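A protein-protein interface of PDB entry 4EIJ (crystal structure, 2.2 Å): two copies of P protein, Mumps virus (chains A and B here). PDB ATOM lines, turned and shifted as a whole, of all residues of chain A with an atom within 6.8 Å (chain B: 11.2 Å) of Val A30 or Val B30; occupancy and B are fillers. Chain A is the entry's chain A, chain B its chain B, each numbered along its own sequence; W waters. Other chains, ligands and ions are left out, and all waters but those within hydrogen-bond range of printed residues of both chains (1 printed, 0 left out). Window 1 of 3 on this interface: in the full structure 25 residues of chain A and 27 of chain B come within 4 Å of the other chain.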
ATOM      1  N   GLN A  25      27.914  -5.213   6.205  1.00  0.00           N
ATOM      2  CA  GLN A  25      27.645  -4.813   7.581  1.00  0.00           C
ATOM      3  C   GLN A  25      26.365  -3.995   7.654  1.00  0.00           C
ATOM      4  O   GLN A  25      25.568  -4.180   8.568  1.00  0.00           O
ATOM      5  CB  GLN A  25      28.779  -3.964   8.153  1.00  0.00           C
ATOM      6  CG  GLN A  25      30.132  -4.615   8.210  1.00  0.00           C
ATOM      7  CD  GLN A  25      31.194  -3.649   8.717  1.00  0.00           C
ATOM      8  OE1 GLN A  25      32.288  -3.546   8.149  1.00  0.00           O
ATOM      9  NE2 GLN A  25      30.866  -2.922   9.784  1.00  0.00           N
ATOM     10  N   LYS A  26      26.178  -3.085   6.699  1.00  0.00           N
ATOM     11  CA  LYS A  26      24.990  -2.221   6.699  1.00  0.00           C
ATOM     12  C   LYS A  26      23.732  -3.007   6.357  1.00  0.00           C
ATOM     13  O   LYS A  26      22.677  -2.770   6.932  1.00  0.00           O
ATOM     14  CB  LYS A  26      25.142  -1.043   5.735  1.00  0.00           C
ATOM     15  CG  LYS A  26      26.046   0.064   6.236  1.00  0.00           C
ATOM     16  CD  LYS A  26      26.351   1.049   5.116  1.00  0.00           C
ATOM     17  CE  LYS A  26      27.422   2.048   5.519  1.00  0.00           C
ATOM     18  NZ  LYS A  26      26.965   2.897   6.644  1.00  0.00           N
ATOM     19  N   VAL A  27      23.850  -3.948   5.423  1.00  0.00           N
ATOM     20  CA  VAL A  27      22.718  -4.802   5.094  1.00  0.00           C
ATOM     21  C   VAL A  27      22.316  -5.609   6.331  1.00  0.00           C
ATOM     22  O   VAL A  27      21.132  -5.736   6.640  1.00  0.00           O
ATOM     23  CB  VAL A  27      23.021  -5.721   3.903  1.00  0.00           C
ATOM     24  CG1 VAL A  27      21.935  -6.763   3.736  1.00  0.00           C
ATOM     25  CG2 VAL A  27      23.160  -4.894   2.636  1.00  0.00           C
ATOM     26  N   ASP A  28      23.310  -6.130   7.049  1.00  0.00           N
ATOM     27  CA  ASP A  28      23.051  -6.828   8.304  1.00  0.00           C
ATOM     28  C   ASP A  28      22.240  -5.969   9.293  1.00  0.00           C
ATOM     29  O   ASP A  28      21.360  -6.486   9.981  1.00  0.00           O
ATOM     30  CB  ASP A  28      24.358  -7.291   8.963  1.00  0.00           C
ATOM     31  CG  ASP A  28      25.002  -8.472   8.241  1.00  0.00           C
ATOM     32  OD1 ASP A  28      24.309  -9.148   7.450  1.00  0.00           O
ATOM     33  OD2 ASP A  28      26.200  -8.739   8.480  1.00  0.00           O
ATOM     34  N   LYS A  29      22.541  -4.674   9.380  1.00  0.00           N
ATOM     35  CA  LYS A  29      21.818  -3.804  10.326  1.00  0.00           C
ATOM     36  C   LYS A  29      20.376  -3.584   9.879  1.00  0.00           C
ATOM     37  O   LYS A  29      19.471  -3.531  10.697  1.00  0.00           O
ATOM     38  CB  LYS A  29      22.512  -2.452  10.519  1.00  0.00           C
ATOM     39  CG  LYS A  29      23.865  -2.529  11.199  1.00  0.00           C
ATOM     40  CD  LYS A  29      24.432  -1.142  11.465  1.00  0.00           C
ATOM     41  CE  LYS A  29      25.955  -1.169  11.560  1.00  0.00           C
ATOM     42  NZ  LYS A  29      26.436  -2.117  12.602  1.00  0.00           N
ATOM     43  N   VAL A  30      20.169  -3.450   8.577  1.00  0.00           N
ATOM     44  CA  VAL A  30      18.821  -3.345   8.051  1.00  0.00           C
ATOM     45  C   VAL A  30      18.050  -4.633   8.327  1.00  0.00           C
ATOM     46  O   VAL A  30      16.935  -4.586   8.828  1.00  0.00           O
ATOM     47  CB  VAL A  30      18.815  -3.027   6.550  1.00  0.00           C
ATOM     48  CG1 VAL A  30      17.420  -3.218   5.988  1.00  0.00           C
ATOM     49  CG2 VAL A  30      19.291  -1.601   6.325  1.00  0.00           C
ATOM     50  N   LEU A  31      18.657  -5.777   8.020  1.00  0.00           N
ATOM     51  CA  LEU A  31      18.036  -7.070   8.303  1.00  0.00           C
ATOM     52  C   LEU A  31      17.566  -7.181   9.746  1.00  0.00           C
ATOM     53  O   LEU A  31      16.459  -7.653  10.004  1.00  0.00           O
ATOM     54  CB  LEU A  31      18.996  -8.225   8.000  1.00  0.00           C
ATOM     55  CG  LEU A  31      18.771  -8.904   6.657  1.00  0.00           C
ATOM     56  CD1 LEU A  31      19.684 -10.114   6.507  1.00  0.00           C
ATOM     57  CD2 LEU A  31      17.296  -9.286   6.525  1.00  0.00           C
ATOM     58  N   ALA A  32      18.419  -6.762  10.680  1.00  0.00           N
ATOM     59  CA  ALA A  32      18.101  -6.838  12.104  1.00  0.00           C
ATOM     60  C   ALA A  32      16.817  -6.079  12.477  1.00  0.00           C
ATOM     61  O   ALA A  32      16.305  -6.227  13.582  1.00  0.00           O
ATOM     62  CB  ALA A  32      19.290  -6.350  12.951  1.00  0.00           C
ATOM     63  N   GLN A  33      16.299  -5.281  11.547  1.00  0.00           N
ATOM     64  CA  GLN A  33      15.036  -4.563  11.747  1.00  0.00           C
ATOM     65  C   GLN A  33      13.795  -5.436  11.508  1.00  0.00           C
ATOM     66  O   GLN A  33      12.682  -5.048  11.859  1.00  0.00           O
ATOM     67  CB  GLN A  33      14.980  -3.345  10.829  1.00  0.00           C
ATOM     68  CG  GLN A  33      14.146  -2.187  11.365  1.00  0.00           C
ATOM     69  CD  GLN A  33      14.744  -1.564  12.610  1.00  0.00           C
ATOM     70  OE1 GLN A  33      15.934  -1.733  12.899  1.00  0.00           O
ATOM     71  NE2 GLN A  33      13.920  -0.839  13.357  1.00  0.00           N
ATOM     72  N   GLY A  34      13.989  -6.610  10.914  1.00  0.00           N
ATOM     73  CA  GLY A  34      12.892  -7.487  10.550  1.00  0.00           C
ATOM     74  C   GLY A  34      12.036  -7.841  11.742  1.00  0.00           C
ATOM     75  O   GLY A  34      10.802  -7.777  11.688  1.00  0.00           O
ATOM     76  N   HIS B  22      26.734 -13.872  -0.580  1.00  0.00           N
ATOM     77  CA  HIS B  22      26.251 -13.617   0.772  1.00  0.00           C
ATOM     78  C   HIS B  22      25.362 -12.375   0.807  1.00  0.00           C
ATOM     79  O   HIS B  22      24.295 -12.388   1.416  1.00  0.00           O
ATOM     80  CB  HIS B  22      27.421 -13.483   1.743  1.00  0.00           C
ATOM     81  CG  HIS B  22      28.285 -14.702   1.802  1.00  0.00           C
ATOM     82  ND1 HIS B  22      29.641 -14.647   2.053  1.00  0.00           N
ATOM     83  CD2 HIS B  22      27.989 -16.010   1.613  1.00  0.00           C
ATOM     84  CE1 HIS B  22      30.137 -15.872   2.035  1.00  0.00           C
ATOM     85  NE2 HIS B  22      29.155 -16.716   1.765  1.00  0.00           N
ATOM     86  N   LEU B  23      25.807 -11.321   0.131  1.00  0.00           N
ATOM     87  CA  LEU B  23      25.016 -10.115  -0.045  1.00  0.00           C
ATOM     88  C   LEU B  23      23.674 -10.413  -0.694  1.00  0.00           C
ATOM     89  O   LEU B  23      22.651  -9.877  -0.275  1.00  0.00           O
ATOM     90  CB  LEU B  23      25.776  -9.085  -0.873  1.00  0.00           C
ATOM     91  CG  LEU B  23      26.570  -8.053  -0.073  1.00  0.00           C
ATOM     92  CD1 LEU B  23      27.560  -7.306  -0.968  1.00  0.00           C
ATOM     93  CD2 LEU B  23      25.632  -7.079   0.599  1.00  0.00           C
ATOM     94  N   GLU B  24      23.669 -11.277  -1.706  1.00  0.00           N
ATOM     95  CA  GLU B  24      22.412 -11.629  -2.362  1.00  0.00           C
ATOM     96  C   GLU B  24      21.444 -12.367  -1.430  1.00  0.00           C
ATOM     97  O   GLU B  24      20.233 -12.145  -1.472  1.00  0.00           O
ATOM     98  CB  GLU B  24      22.653 -12.439  -3.633  1.00  0.00           C
ATOM     99  CG  GLU B  24      22.703 -11.562  -4.871  1.00  0.00           C
ATOM    100  CD  GLU B  24      22.337 -12.305  -6.138  1.00  0.00           C
ATOM    101  OE1 GLU B  24      22.116 -11.634  -7.168  1.00  0.00           O
ATOM    102  OE2 GLU B  24      22.263 -13.552  -6.108  1.00  0.00           O
ATOM    103  N   GLN B  25      21.979 -13.247  -0.596  1.00  0.00           N
ATOM    104  CA  GLN B  25      21.142 -13.971   0.349  1.00  0.00           C
ATOM    105  C   GLN B  25      20.545 -12.997   1.369  1.00  0.00           C
ATOM    106  O   GLN B  25      19.375 -13.101   1.722  1.00  0.00           O
ATOM    107  CB  GLN B  25      21.938 -15.072   1.037  1.00  0.00           C
ATOM    108  CG  GLN B  25      22.464 -16.149   0.086  1.00  0.00           C
ATOM    109  CD  GLN B  25      21.424 -17.201  -0.275  1.00  0.00           C
ATOM    110  OE1 GLN B  25      20.613 -17.604   0.559  1.00  0.00           O
ATOM    111  NE2 GLN B  25      21.461 -17.667  -1.520  1.00  0.00           N
ATOM    112  N   LYS B  26      21.349 -12.044   1.827  1.00  0.00           N
ATOM    113  CA  LYS B  26      20.877 -11.049   2.778  1.00  0.00           C
ATOM    114  C   LYS B  26      19.864 -10.116   2.131  1.00  0.00           C
ATOM    115  O   LYS B  26      18.785  -9.891   2.672  1.00  0.00           O
ATOM    116  CB  LYS B  26      22.041 -10.245   3.346  1.00  0.00           C
ATOM    117  CG  LYS B  26      22.995 -11.076   4.199  1.00  0.00           C
ATOM    118  CD  LYS B  26      24.276 -10.291   4.480  1.00  0.00           C
ATOM    119  CE  LYS B  26      25.401 -11.200   4.950  1.00  0.00           C
ATOM    120  NZ  LYS B  26      25.123 -11.764   6.295  1.00  0.00           N
ATOM    121  N   VAL B  27      20.202  -9.580   0.963  1.00  0.00           N
ATOM    122  CA  VAL B  27      19.275  -8.685   0.274  1.00  0.00           C
ATOM    123  C   VAL B  27      17.949  -9.376  -0.049  1.00  0.00           C
ATOM    124  O   VAL B  27      16.893  -8.762   0.064  1.00  0.00           O
ATOM    125  CB  VAL B  27      19.900  -8.058  -0.973  1.00  0.00           C
ATOM    126  CG1 VAL B  27      18.832  -7.428  -1.852  1.00  0.00           C
ATOM    127  CG2 VAL B  27      20.941  -7.038  -0.555  1.00  0.00           C
ATOM    128  N   ASP B  28      17.993 -10.653  -0.422  1.00  0.00           N
ATOM    129  CA  ASP B  28      16.758 -11.408  -0.604  1.00  0.00           C
ATOM    130  C   ASP B  28      15.915 -11.349   0.667  1.00  0.00           C
ATOM    131  O   ASP B  28      14.688 -11.218   0.600  1.00  0.00           O
ATOM    132  CB  ASP B  28      17.022 -12.868  -0.995  1.00  0.00           C
ATOM    133  CG  ASP B  28      17.469 -13.024  -2.452  1.00  0.00           C
ATOM    134  OD1 ASP B  28      17.448 -12.025  -3.207  1.00  0.00           O
ATOM    135  OD2 ASP B  28      17.847 -14.154  -2.839  1.00  0.00           O
ATOM    136  N   LYS B  29      16.561 -11.455   1.828  1.00  0.00           N
ATOM    137  CA  LYS B  29      15.804 -11.401   3.079  1.00  0.00           C
ATOM    138  C   LYS B  29      15.171 -10.030   3.296  1.00  0.00           C
ATOM    139  O   LYS B  29      14.044  -9.937   3.780  1.00  0.00           O
ATOM    140  CB  LYS B  29      16.657 -11.800   4.283  1.00  0.00           C
ATOM    141  CG  LYS B  29      16.936 -13.284   4.366  1.00  0.00           C
ATOM    142  CD  LYS B  29      17.933 -13.582   5.473  1.00  0.00           C
ATOM    143  CE  LYS B  29      18.400 -15.030   5.421  1.00  0.00           C
ATOM    144  NZ  LYS B  29      19.421 -15.326   6.468  1.00  0.00           N
ATOM    145  N   VAL B  30      15.889  -8.965   2.943  1.00  0.00           N
ATOM    146  CA  VAL B  30      15.323  -7.627   3.082  1.00  0.00           C
ATOM    147  C   VAL B  30      14.131  -7.444   2.137  1.00  0.00           C
ATOM    148  O   VAL B  30      13.143  -6.786   2.482  1.00  0.00           O
ATOM    149  CB  VAL B  30      16.357  -6.523   2.846  1.00  0.00           C
ATOM    150  CG1 VAL B  30      15.702  -5.146   3.017  1.00  0.00           C
ATOM    151  CG2 VAL B  30      17.523  -6.684   3.800  1.00  0.00           C
ATOM    152  N   LEU B  31      14.228  -8.030   0.948  1.00  0.00           N
ATOM    153  CA  LEU B  31      13.112  -8.020  -0.001  1.00  0.00           C
ATOM    154  C   LEU B  31      11.863  -8.701   0.560  1.00  0.00           C
ATOM    155  O   LEU B  31      10.732  -8.236   0.353  1.00  0.00           O
ATOM    156  CB  LEU B  31      13.517  -8.679  -1.322  1.00  0.00           C
ATOM    157  CG  LEU B  31      14.361  -7.825  -2.270  1.00  0.00           C
ATOM    158  CD1 LEU B  31      14.867  -8.653  -3.445  1.00  0.00           C
ATOM    159  CD2 LEU B  31      13.539  -6.643  -2.760  1.00  0.00           C
ATOM    160  N   ALA B  32      12.056  -9.812   1.261  1.00  0.00           N
ATOM    161  CA  ALA B  32      10.924 -10.469   1.920  1.00  0.00           C
ATOM    162  C   ALA B  32      10.346  -9.572   3.018  1.00  0.00           C
ATOM    163  O   ALA B  32       9.134  -9.542   3.246  1.00  0.00           O
ATOM    164  CB  ALA B  32      11.337 -11.827   2.478  1.00  0.00           C
ATOM    165  N   GLN B  33      11.219  -8.829   3.693  1.00  0.00           N
ATOM    166  CA  GLN B  33      10.773  -7.852   4.680  1.00  0.00           C
ATOM    167  C   GLN B  33       9.837  -6.859   4.016  1.00  0.00           C
ATOM    168  O   GLN B  33       8.771  -6.524   4.551  1.00  0.00           O
ATOM    169  CB  GLN B  33      11.962  -7.113   5.274  1.00  0.00           C
ATOM    170  CG  GLN B  33      12.143  -7.325   6.751  1.00  0.00           C
ATOM    171  CD  GLN B  33      13.533  -6.936   7.224  1.00  0.00           C
ATOM    172  OE1 GLN B  33      14.276  -7.777   7.730  1.00  0.00           O
ATOM    173  NE2 GLN B  33      13.887  -5.657   7.077  1.00  0.00           N
ATOM    174  N   GLY B  34      10.238  -6.402   2.834  1.00  0.00           N
ATOM    175  CA  GLY B  34       9.464  -5.428   2.086  1.00  0.00           C
ATOM    176  C   GLY B  34       8.080  -5.914   1.702  1.00  0.00           C
ATOM    177  O   GLY B  34       7.132  -5.124   1.653  1.00  0.00           O
ATOM    178  N   SER B  35       7.952  -7.212   1.432  1.00  0.00           N
ATOM    179  CA  SER B  35       6.667  -7.755   1.004  1.00  0.00           C
ATOM    180  C   SER B  35       5.627  -7.705   2.127  1.00  0.00           C
ATOM    181  O   SER B  35       4.434  -7.650   1.863  1.00  0.00           O
ATOM    182  CB  SER B  35       6.812  -9.171   0.422  1.00  0.00           C
ATOM    183  OG  SER B  35       7.092 -10.130   1.425  1.00  0.00           O
ATOM    184  N   MET B  36       6.067  -7.700   3.381  1.00  0.00           N
ATOM    185  CA  MET B  36       5.102  -7.514   4.446  1.00  0.00           C
ATOM    186  C   MET B  36       4.823  -6.051   4.781  1.00  0.00           C
ATOM    187  O   MET B  36       3.777  -5.742   5.359  1.00  0.00           O
ATOM    188  CB  MET B  36       5.367  -8.386   5.682  1.00  0.00           C
ATOM    189  CG  MET B  36       6.619  -8.125   6.467  1.00  0.00           C
ATOM    190  SD  MET B  36       6.572  -9.215   7.910  1.00  0.00           S
ATOM    191  CE  MET B  36       5.955 -10.707   7.146  1.00  0.00           C
ATOM    192  N   VAL B  37       5.720  -5.147   4.388  1.00  0.00           N
ATOM    193  CA  VAL B  37       5.387  -3.727   4.458  1.00  0.00           C
ATOM    194  C   VAL B  37       4.203  -3.503   3.515  1.00  0.00           C
ATOM    195  O   VAL B  37       3.298  -2.718   3.787  1.00  0.00           O
ATOM    196  CB  VAL B  37       6.563  -2.806   4.044  1.00  0.00           C
ATOM    197  CG1 VAL B  37       6.116  -1.357   4.022  1.00  0.00           C
ATOM    198  CG2 VAL B  37       7.747  -2.973   4.991  1.00  0.00           C
ATOM    199  N   THR B  38       4.228  -4.224   2.403  1.00  0.00           N
ATOM    200  CA  THR B  38       3.174  -4.163   1.407  1.00  0.00           C
ATOM    201  C   THR B  38       1.874  -4.698   1.988  1.00  0.00           C
ATOM    202  O   THR B  38       0.799  -4.169   1.709  1.00  0.00           O
ATOM    203  CB  THR B  38       3.560  -4.977   0.161  1.00  0.00           C
ATOM    204  OG1 THR B  38       4.561  -4.264  -0.576  1.00  0.00           O
ATOM    205  CG2 THR B  38       2.357  -5.218  -0.728  1.00  0.00           C
ATOM    206  N   ILE B  40       1.259  -4.623   5.252  1.00  0.00           N
ATOM    207  CA  ILE B  40       0.904  -3.628   6.257  1.00  0.00           C
ATOM    208  C   ILE B  40       0.095  -2.493   5.631  1.00  0.00           C
ATOM    209  O   ILE B  40      -0.938  -2.085   6.164  1.00  0.00           O
ATOM    210  CB  ILE B  40       2.134  -3.072   6.974  1.00  0.00           C
ATOM    211  CG1 ILE B  40       2.726  -4.128   7.912  1.00  0.00           C
ATOM    212  CG2 ILE B  40       1.766  -1.822   7.761  1.00  0.00           C
ATOM    213  CD1 ILE B  40       4.190  -3.854   8.297  1.00  0.00           C
HETATM  214  O   HOH W   1       9.783  -9.132   8.657  1.00  0.00           O
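Val A27 touches just these residues of chain B: Leu B23 (3.9 Å) and Lys B26 (3.5 Å). Of the printed residues of chain B, Asp A28 touches Lys B26. No residue of chain B comes within 4 Å of Ala A32. No residue of chain B comes within 4 Å of Gln A33. His B22 touches none of the printed residues of chain A. Printed residues of chain A within 4 Å of Lys B29: Leu A31. Of the printed residues of chain A, Val B30 touches Val A30 and Leu A31. The nearest residue of chain B that does not touch Val A30 is Lys B26 (7.6 Å). The nearest residue of chain A that does not touch Val B30 is Val A27 (4.4 Å). The nearest printed residue of chain A that does not touch Leu B23 is Gln A25 (6.3 Å).
Val A30 touches Gln B33, but with the chains exchanged Gln A33 does not touch Val B30 (8.0 Å). Leu A31 touches Lys B26, but with the chains exchanged Lys A26 does not touch Leu B31 (11.6 Å). Leu A31 touches Lys B29, but with the chains exchanged Lys A29 does not touch Leu B31 (11.7 Å). Gly A34 touches Gln B33, but with the chains exchanged Gln A33 does not touch Gly B34 (9.4 Å). Positions printed for both chains: 25, 26, 27, 28, 29, 30, 31, 32, 33 and 34. Of the 10 pairs that touch across the chains among the printed residues, 1 has its exchanged pair printed and touching as well.
Hydrophobic or aromatic side chains of chain B within 4 Å of the printed part of chain A: Leu B23 and Val B30. Of the 10 printed residues of chain A, 5 touch a printed residue of chain B. Among the printed residues, Asp or Glu carboxylates within 4 Å of a Lys or Arg side-chain nitrogen of the other chain: Asp A28 with Lys B26.
Among the printed residues, pairs that only touch across the chains: Val A27 with Leu B23, Val A27 with Lys B26, Val A30 with Val B30, Val A30 with Gln B33, Leu A31 with Lys B26, Leu A31 with Lys B29 and Leu A31 with Val B30.
OE1 of Gln B33 sits close to O of Leu A31 (3.2 Å). The side-chain carboxylate (OD1) of Asp A28 is in salt-bridge range of the side-chain amino group (NZ) of Lys B26, at 3.0 Å. The backbone NH (N) of Gly A34 sits close to the side-chain amide oxygen (OE1) of Gln B33.
Water W1 lies within hydrogen-bond range of SD of Met B36 and O of Gly A34.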
